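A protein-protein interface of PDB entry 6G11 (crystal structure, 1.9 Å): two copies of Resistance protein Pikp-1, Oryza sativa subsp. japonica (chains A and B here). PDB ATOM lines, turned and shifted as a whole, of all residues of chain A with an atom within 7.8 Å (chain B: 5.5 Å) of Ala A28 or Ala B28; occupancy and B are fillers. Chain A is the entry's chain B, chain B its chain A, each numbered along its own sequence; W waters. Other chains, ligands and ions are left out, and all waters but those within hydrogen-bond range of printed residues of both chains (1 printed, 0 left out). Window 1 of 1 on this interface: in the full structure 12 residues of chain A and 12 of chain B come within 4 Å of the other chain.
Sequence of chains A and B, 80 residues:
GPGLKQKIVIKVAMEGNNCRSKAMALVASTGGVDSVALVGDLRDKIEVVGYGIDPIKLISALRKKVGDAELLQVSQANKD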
ATOM      1  N   ARG A  20      26.027 -15.400   4.522  1.00  0.00           N
ATOM      2  CA  ARG A  20      25.192 -14.829   5.587  1.00  0.00           C
ATOM      3  C   ARG A  20      24.629 -13.492   5.138  1.00  0.00           C
ATOM      4  O   ARG A  20      23.403 -13.294   5.129  1.00  0.00           O
ATOM      5  CB  ARG A  20      25.961 -14.628   6.910  1.00  0.00           C
ATOM      6  CG  ARG A  20      25.672 -15.693   7.923  1.00  0.00           C
ATOM      7  CD  ARG A  20      26.392 -15.654   9.279  1.00  0.00           C
ATOM      8  NE  ARG A  20      26.239 -16.952   9.922  1.00  0.00           N
ATOM      9  CZ  ARG A  20      27.099 -17.978   9.847  1.00  0.00           C
ATOM     10  NH1 ARG A  20      26.788 -19.137  10.436  1.00  0.00           N
ATOM     11  NH2 ARG A  20      28.229 -17.904   9.148  1.00  0.00           N
ATOM     12  N   SER A  21      25.544 -12.609   4.769  1.00  0.00           N
ATOM     13  CA  SER A  21      25.184 -11.266   4.399  1.00  0.00           C
ATOM     14  C   SER A  21      24.352 -11.227   3.111  1.00  0.00           C
ATOM     15  O   SER A  21      23.446 -10.417   2.990  1.00  0.00           O
ATOM     16  CB  SER A  21      26.442 -10.422   4.263  1.00  0.00           C
ATOM     17  OG  SER A  21      26.951 -10.759   3.040  1.00  0.00           O
ATOM     18  N   LYS A  22      24.659 -12.105   2.162  1.00  0.00           N
ATOM     19  CA  LYS A  22      23.886 -12.179   0.920  1.00  0.00           C
ATOM     20  C   LYS A  22      22.475 -12.666   1.193  1.00  0.00           C
ATOM     21  O   LYS A  22      21.515 -12.140   0.631  1.00  0.00           O
ATOM     22  CB  LYS A  22      24.562 -13.093  -0.091  1.00  0.00           C
ATOM     23  CG  LYS A  22      25.727 -12.382  -0.825  1.00  0.00           C
ATOM     24  CD  LYS A  22      26.817 -13.353  -1.279  1.00  0.00           C
ATOM     25  CE  LYS A  22      26.280 -14.198  -2.428  1.00  0.00           C
ATOM     26  NZ  LYS A  22      27.157 -15.381  -2.678  1.00  0.00           N
ATOM     27  N   ALA A  23      22.349 -13.679   2.033  1.00  0.00           N
ATOM     28  CA  ALA A  23      21.028 -14.200   2.369  1.00  0.00           C
ATOM     29  C   ALA A  23      20.202 -13.138   3.105  1.00  0.00           C
ATOM     30  O   ALA A  23      19.049 -12.918   2.764  1.00  0.00           O
ATOM     31  CB  ALA A  23      21.152 -15.472   3.215  1.00  0.00           C
ATOM     32  N   MET A  24      20.817 -12.489   4.104  1.00  0.00           N
ATOM     33  CA  MET A  24      20.150 -11.457   4.902  1.00  0.00           C
ATOM     34  C   MET A  24      19.669 -10.331   3.967  1.00  0.00           C
ATOM     35  O   MET A  24      18.543  -9.892   4.059  1.00  0.00           O
ATOM     36  CB  MET A  24      21.097 -10.901   5.965  1.00  0.00           C
ATOM     37  CG  MET A  24      21.352 -11.809   7.146  1.00  0.00           C
ATOM     38  SD  MET A  24      19.958 -11.774   8.315  1.00  0.00           S
ATOM     39  CE  MET A  24      20.356 -10.226   9.150  1.00  0.00           C
ATOM     40  N   ALA A  25      20.522  -9.896   3.048  1.00  0.00           N
ATOM     41  CA  ALA A  25      20.160  -8.851   2.118  1.00  0.00           C
ATOM     42  C   ALA A  25      19.008  -9.244   1.191  1.00  0.00           C
ATOM     43  O   ALA A  25      18.078  -8.453   0.960  1.00  0.00           O
ATOM     44  CB  ALA A  25      21.376  -8.419   1.297  1.00  0.00           C
ATOM     45  N   LEU A  26      19.057 -10.462   0.672  1.00  0.00           N
ATOM     46  CA  LEU A  26      17.999 -10.941  -0.207  1.00  0.00           C
ATOM     47  C   LEU A  26      16.664 -10.989   0.537  1.00  0.00           C
ATOM     48  O   LEU A  26      15.643 -10.453   0.062  1.00  0.00           O
ATOM     49  CB  LEU A  26      18.358 -12.327  -0.769  1.00  0.00           C
ATOM     50  CG  LEU A  26      17.375 -12.877  -1.841  1.00  0.00           C
ATOM     51  CD1 LEU A  26      18.025 -13.969  -2.632  1.00  0.00           C
ATOM     52  CD2 LEU A  26      16.135 -13.460  -1.193  1.00  0.00           C
ATOM     53  N   VAL A  27      16.672 -11.593   1.721  1.00  0.00           N
ATOM     54  CA  VAL A  27      15.432 -11.670   2.499  1.00  0.00           C
ATOM     55  C   VAL A  27      14.924 -10.261   2.855  1.00  0.00           C
ATOM     56  O   VAL A  27      13.744  -9.959   2.690  1.00  0.00           O
ATOM     57  CB  VAL A  27      15.591 -12.516   3.764  1.00  0.00           C
ATOM     58  CG1 VAL A  27      14.297 -12.484   4.602  1.00  0.00           C
ATOM     59  CG2 VAL A  27      15.913 -13.958   3.382  1.00  0.00           C
ATOM     60  N   ALA A  28      15.833  -9.399   3.314  1.00  0.00           N
ATOM     61  CA  ALA A  28      15.469  -8.051   3.720  1.00  0.00           C
ATOM     62  C   ALA A  28      14.880  -7.206   2.588  1.00  0.00           C
ATOM     63  O   ALA A  28      14.098  -6.296   2.843  1.00  0.00           O
ATOM     64  CB  ALA A  28      16.658  -7.331   4.349  1.00  0.00           C
ATOM     65  N   SER A  29      15.229  -7.528   1.347  1.00  0.00           N
ATOM     66  CA  SER A  29      14.754  -6.794   0.188  1.00  0.00           C
ATOM     67  C   SER A  29      13.364  -7.233  -0.230  1.00  0.00           C
ATOM     68  O   SER A  29      12.776  -6.615  -1.109  1.00  0.00           O
ATOM     69  CB  SER A  29      15.720  -7.003  -0.997  1.00  0.00           C
ATOM     70  OG  SER A  29      15.560  -8.324  -1.487  1.00  0.00           O
ATOM     71  N   THR A  30      12.825  -8.285   0.389  1.00  0.00           N
ATOM     72  CA  THR A  30      11.549  -8.881  -0.017  1.00  0.00           C
ATOM     73  C   THR A  30      10.368  -8.018   0.420  1.00  0.00           C
ATOM     74  O   THR A  30      10.363  -7.467   1.528  1.00  0.00           O
ATOM     75  CB  THR A  30      11.438 -10.311   0.550  1.00  0.00           C
ATOM     76  OG1 THR A  30      12.527 -11.101   0.023  1.00  0.00           O
ATOM     77  CG2 THR A  30      10.108 -10.972   0.216  1.00  0.00           C
ATOM     78  N   GLY A  31       9.358  -7.895  -0.453  1.00  0.00           N
ATOM     79  CA  GLY A  31       8.171  -7.116  -0.160  1.00  0.00           C
ATOM     80  C   GLY A  31       7.478  -7.633   1.106  1.00  0.00           C
ATOM     81  O   GLY A  31       7.434  -8.832   1.340  1.00  0.00           O
ATOM     82  N   GLY A  32       7.010  -6.709   1.931  1.00  0.00           N
ATOM     83  CA  GLY A  32       6.286  -7.030   3.179  1.00  0.00           C
ATOM     84  C   GLY A  32       7.131  -7.315   4.416  1.00  0.00           C
ATOM     85  O   GLY A  32       6.606  -7.590   5.476  1.00  0.00           O
ATOM     86  N   VAL A  33       8.460  -7.280   4.272  1.00  0.00           N
ATOM     87  CA  VAL A  33       9.371  -7.594   5.403  1.00  0.00           C
ATOM     88  C   VAL A  33       9.405  -6.464   6.430  1.00  0.00           C
ATOM     89  O   VAL A  33       9.652  -5.305   6.098  1.00  0.00           O
ATOM     90  CB  VAL A  33      10.758  -7.951   4.890  1.00  0.00           C
ATOM     91  CG1 VAL A  33      11.794  -8.020   6.015  1.00  0.00           C
ATOM     92  CG2 VAL A  33      10.652  -9.262   4.170  1.00  0.00           C
ATOM     93  N   ASP A  34       9.157  -6.810   7.680  1.00  0.00           N
ATOM     94  CA  ASP A  34       9.341  -5.888   8.821  1.00  0.00           C
ATOM     95  C   ASP A  34      10.719  -6.080   9.480  1.00  0.00           C
ATOM     96  O   ASP A  34      11.326  -5.076   9.871  1.00  0.00           O
ATOM     97  CB  ASP A  34       8.313  -6.105   9.916  1.00  0.00           C
ATOM     98  CG  ASP A  34       6.872  -5.782   9.500  1.00  0.00           C
ATOM     99  OD1 ASP A  34       6.684  -5.042   8.525  1.00  0.00           O
ATOM    100  OD2 ASP A  34       5.929  -6.235  10.207  1.00  0.00           O
ATOM    101  N   SER A  35      11.203  -7.326   9.612  1.00  0.00           N
ATOM    102  CA  SER A  35      12.516  -7.565  10.201  1.00  0.00           C
ATOM    103  C   SER A  35      13.139  -8.840   9.712  1.00  0.00           C
ATOM    104  O   SER A  35      12.421  -9.781   9.371  1.00  0.00           O
ATOM    105  CB  SER A  35      12.426  -7.629  11.745  1.00  0.00           C
ATOM    106  OG  SER A  35      11.625  -8.739  12.195  1.00  0.00           O
ATOM    107  N   VAL A  36      14.471  -8.884   9.716  1.00  0.00           N
ATOM    108  CA  VAL A  36      15.256 -10.067   9.514  1.00  0.00           C
ATOM    109  C   VAL A  36      16.318 -10.137  10.615  1.00  0.00           C
ATOM    110  O   VAL A  36      16.918  -9.131  10.962  1.00  0.00           O
ATOM    111  CB  VAL A  36      15.935 -10.114   8.108  1.00  0.00           C
ATOM    112  CG1 VAL A  36      14.934  -9.976   6.985  1.00  0.00           C
ATOM    113  CG2 VAL A  36      16.922  -8.989   7.927  1.00  0.00           C
ATOM    114  N   LEU A  38      19.516 -12.900  12.261  1.00  0.00           N
ATOM    115  CA  LEU A  38      20.267 -14.143  12.329  1.00  0.00           C
ATOM    116  C   LEU A  38      20.079 -14.727  13.680  1.00  0.00           C
ATOM    117  O   LEU A  38      20.377 -14.088  14.625  1.00  0.00           O
ATOM    118  CB  LEU A  38      21.750 -13.908  12.118  1.00  0.00           C
ATOM    119  CG  LEU A  38      22.179 -13.603  10.725  1.00  0.00           C
ATOM    120  CD1 LEU A  38      23.657 -13.162  10.771  1.00  0.00           C
ATOM    121  CD2 LEU A  38      21.953 -14.836   9.831  1.00  0.00           C
ATOM    122  N   ILE A  46      17.776 -17.526   9.499  1.00  0.00           N
ATOM    123  CA  ILE A  46      17.186 -16.218   9.348  1.00  0.00           C
ATOM    124  C   ILE A  46      15.718 -16.282   9.762  1.00  0.00           C
ATOM    125  O   ILE A  46      14.955 -17.093   9.217  1.00  0.00           O
ATOM    126  CB  ILE A  46      17.301 -15.715   7.915  1.00  0.00           C
ATOM    127  CG1 ILE A  46      18.774 -15.633   7.556  1.00  0.00           C
ATOM    128  CG2 ILE A  46      16.614 -14.332   7.796  1.00  0.00           C
ATOM    129  CD1 ILE A  46      19.045 -15.088   6.190  1.00  0.00           C
ATOM    130  N   VAL A  48      12.390 -14.084   9.840  1.00  0.00           N
ATOM    131  CA  VAL A  48      11.813 -12.986   9.082  1.00  0.00           C
ATOM    132  C   VAL A  48      10.402 -12.812   9.570  1.00  0.00           C
ATOM    133  O   VAL A  48       9.647 -13.795   9.665  1.00  0.00           O
ATOM    134  CB  VAL A  48      11.931 -13.105   7.522  1.00  0.00           C
ATOM    135  CG1 VAL A  48      11.320 -14.302   6.967  1.00  0.00           C
ATOM    136  CG2 VAL A  48      11.431 -11.868   6.779  1.00  0.00           C
ATOM    137  N   LEU A  58      10.392 -17.418  -1.531  1.00  0.00           N
ATOM    138  CA  LEU A  58      11.567 -16.927  -0.834  1.00  0.00           C
ATOM    139  C   LEU A  58      12.672 -17.988  -0.793  1.00  0.00           C
ATOM    140  O   LEU A  58      13.824 -17.694  -1.071  1.00  0.00           O
ATOM    141  CB  LEU A  58      11.164 -16.485   0.580  1.00  0.00           C
ATOM    142  CG  LEU A  58      12.220 -15.864   1.468  1.00  0.00           C
ATOM    143  CD1 LEU A  58      12.848 -14.702   0.734  1.00  0.00           C
ATOM    144  CD2 LEU A  58      11.622 -15.374   2.767  1.00  0.00           C
ATOM    145  N   SER B  21      12.887  -1.236   0.686  1.00  0.00           N
ATOM    146  CA  SER B  21      13.495  -2.530   0.419  1.00  0.00           C
ATOM    147  C   SER B  21      14.976  -2.388   0.068  1.00  0.00           C
ATOM    148  O   SER B  21      15.771  -3.220   0.487  1.00  0.00           O
ATOM    149  CB  SER B  21      12.745  -3.274  -0.675  1.00  0.00           C
ATOM    150  OG  SER B  21      11.455  -3.607  -0.167  1.00  0.00           O
ATOM    151  N   ALA B  23      16.978   0.086   1.120  1.00  0.00           N
ATOM    152  CA  ALA B  23      17.660   0.466   2.353  1.00  0.00           C
ATOM    153  C   ALA B  23      17.827  -0.775   3.265  1.00  0.00           C
ATOM    154  O   ALA B  23      18.911  -0.996   3.766  1.00  0.00           O
ATOM    155  CB  ALA B  23      16.887   1.549   3.102  1.00  0.00           C
ATOM    156  N   MET B  24      16.756  -1.553   3.438  1.00  0.00           N
ATOM    157  CA  MET B  24      16.788  -2.741   4.272  1.00  0.00           C
ATOM    158  C   MET B  24      17.832  -3.722   3.764  1.00  0.00           C
ATOM    159  O   MET B  24      18.621  -4.255   4.532  1.00  0.00           O
ATOM    160  CB  MET B  24      15.398  -3.412   4.325  1.00  0.00           C
ATOM    161  CG  MET B  24      14.347  -2.675   5.134  1.00  0.00           C
ATOM    162  SD  MET B  24      14.679  -2.779   6.905  1.00  0.00           S
ATOM    163  CE  MET B  24      14.103  -4.436   7.256  1.00  0.00           C
ATOM    164  N   ALA B  25      17.874  -3.933   2.454  1.00  0.00           N
ATOM    165  CA  ALA B  25      18.856  -4.823   1.864  1.00  0.00           C
ATOM    166  C   ALA B  25      20.283  -4.338   2.068  1.00  0.00           C
ATOM    167  O   ALA B  25      21.179  -5.140   2.413  1.00  0.00           O
ATOM    168  CB  ALA B  25      18.561  -5.033   0.380  1.00  0.00           C
ATOM    169  N   LEU B  26      20.510  -3.050   1.868  1.00  0.00           N
ATOM    170  CA  LEU B  26      21.840  -2.474   2.055  1.00  0.00           C
ATOM    171  C   LEU B  26      22.290  -2.636   3.495  1.00  0.00           C
ATOM    172  O   LEU B  26      23.392  -3.121   3.758  1.00  0.00           O
ATOM    173  CB  LEU B  26      21.861  -1.000   1.642  1.00  0.00           C
ATOM    174  CG  LEU B  26      23.211  -0.290   1.647  1.00  0.00           C
ATOM    175  CD1 LEU B  26      23.177   0.951   0.770  1.00  0.00           C
ATOM    176  CD2 LEU B  26      23.667   0.067   3.053  1.00  0.00           C
ATOM    177  N   VAL B  27      21.437  -2.261   4.440  1.00  0.00           N
ATOM    178  CA  VAL B  27      21.799  -2.376   5.859  1.00  0.00           C
ATOM    179  C   VAL B  27      22.042  -3.854   6.215  1.00  0.00           C
ATOM    180  O   VAL B  27      23.059  -4.178   6.850  1.00  0.00           O
ATOM    181  CB  VAL B  27      20.742  -1.790   6.800  1.00  0.00           C
ATOM    182  CG1 VAL B  27      21.106  -2.038   8.262  1.00  0.00           C
ATOM    183  CG2 VAL B  27      20.586  -0.304   6.562  1.00  0.00           C
ATOM    184  N   ALA B  28      21.142  -4.735   5.777  1.00  0.00           N
ATOM    185  CA  ALA B  28      21.257  -6.158   6.092  1.00  0.00           C
ATOM    186  C   ALA B  28      22.531  -6.806   5.537  1.00  0.00           C
ATOM    187  O   ALA B  28      23.002  -7.777   6.083  1.00  0.00           O
ATOM    188  CB  ALA B  28      20.015  -6.924   5.620  1.00  0.00           C
ATOM    189  N   SER B  29      23.081  -6.245   4.467  1.00  0.00           N
ATOM    190  CA  SER B  29      24.273  -6.782   3.837  1.00  0.00           C
ATOM    191  C   SER B  29      25.544  -6.326   4.551  1.00  0.00           C
ATOM    192  O   SER B  29      26.616  -6.807   4.220  1.00  0.00           O
ATOM    193  CB  SER B  29      24.334  -6.335   2.361  1.00  0.00           C
ATOM    194  OG  SER B  29      24.677  -4.951   2.316  1.00  0.00           O
ATOM    195  N   THR B  30      25.423  -5.412   5.509  1.00  0.00           N
ATOM    196  CA  THR B  30      26.580  -4.745   6.121  1.00  0.00           C
ATOM    197  C   THR B  30      27.276  -5.670   7.115  1.00  0.00           C
ATOM    198  O   THR B  30      26.619  -6.398   7.864  1.00  0.00           O
ATOM    199  CB  THR B  30      26.141  -3.435   6.814  1.00  0.00           C
ATOM    200  OG1 THR B  30      25.609  -2.569   5.848  1.00  0.00           O
ATOM    201  CG2 THR B  30      27.268  -2.717   7.520  1.00  0.00           C
ATOM    202  N   VAL B  33      26.257  -7.049  11.106  1.00  0.00           N
ATOM    203  CA  VAL B  33      24.802  -6.953  11.354  1.00  0.00           C
ATOM    204  C   VAL B  33      24.204  -8.300  11.736  1.00  0.00           C
ATOM    205  O   VAL B  33      24.354  -9.275  11.029  1.00  0.00           O
ATOM    206  CB  VAL B  33      24.082  -6.350  10.151  1.00  0.00           C
ATOM    207  CG1 VAL B  33      22.563  -6.424  10.318  1.00  0.00           C
ATOM    208  CG2 VAL B  33      24.569  -4.946   9.934  1.00  0.00           C
ATOM    209  N   VAL B  36      17.991  -6.446  11.407  1.00  0.00           N
ATOM    210  CA  VAL B  36      17.486  -5.198  10.873  1.00  0.00           C
ATOM    211  C   VAL B  36      15.968  -5.222  11.016  1.00  0.00           C
ATOM    212  O   VAL B  36      15.310  -6.243  10.707  1.00  0.00           O
ATOM    213  CB  VAL B  36      17.888  -4.923   9.401  1.00  0.00           C
ATOM    214  CG1 VAL B  36      19.371  -4.947   9.188  1.00  0.00           C
ATOM    215  CG2 VAL B  36      17.375  -5.972   8.475  1.00  0.00           C
HETATM  216  O   HOH W   1      11.763  -5.244   2.131  1.00  0.00           O
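The backbone carbonyl oxygen of Leu B26 is in hydrogen-bond range of the side-chain hydroxyl of Ser B29. The side-chain hydroxyl (OG) of Ser A29 sits at hydrogen-bond distance from the backbone carbonyl oxygen (O) of Leu A26, at 2.6 Å.
Of the 21 printed residues of chain A, 9 touch a printed residue of chain B. Of the 11 printed residues of chain B, 7 touch a printed residue of chain A. Among the printed residues, 13 pairs touch across the chains. Among the printed residues, no Asp or Glu carboxylate lies within 4 Å of a Lys or Arg side-chain nitrogen of the other chain.
Of the printed residues of chain B, Ala A25 touches Ala B25, Ala B28 and Ser B29. Of chain B, only Met B24 (3.5 Å) and Ala B28 (3.6 Å) come within 4 Å of Ala A28. Of the printed residues of chain B, Asp A34 touches Met B24. Printed residues of chain B within 4 Å of Val A36: Val B36. Of the printed residues of chain A, Val B36 touches Ser A35 (3.1 Å) and Val A36 (2.9 Å). The nearest printed residue of chain A that does not touch Ser B21 is Ala A28 (4.2 Å).
Among the printed residues, pairs that only touch across the chains: Ser A35 with Val B36 (3.1 Å), Ala A25 with Ala B25 (3.5 Å), Ala A28 with Met B24 (3.5 Å), Ala A28 with Ala B28 (3.6 Å), Ser A21 with Ser B29 (3.6 Å), Met A24 with Ala B28 (3.7 Å), Ser A29 with Ala B25 (3.7 Å), Ala A25 with Ser B29 (3.8 Å), Asp A34 with Met B24 (3.9 Å), Leu A38 with Val B33 (3.96 Å) and Ala A25 with Ala B28 (3.96 Å).
O of Ser A29 lies close to OG of Ser B21. N of Val B36 sits at hydrogen-bond distance from O of Val A36 (2.9 Å).
Ser A21 touches Ser B29, and with the chains exchanged Ser A29 touches Ser B21. Met A24 touches Ala B28, and with the chains exchanged Ala A28 touches Met B24. Ala A28 touches its own counterpart, Ala B28. Val B36 touches its own counterpart, Val A36. Positions printed for both chains: 21, 23, 24, 25, 26, 27, 28, 29, 30, 33 and 36. Of the 13 pairs that touch across the chains among the printed residues, 9 have their exchanged pair printed and touching as well.
Water W1 lies within hydrogen-bond range of the backbone carbonyl oxygen (O) of Ala A28, the backbone carbonyl oxygen (O) of Thr A30 and the side-chain hydroxyl (OG) of Ser B21.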
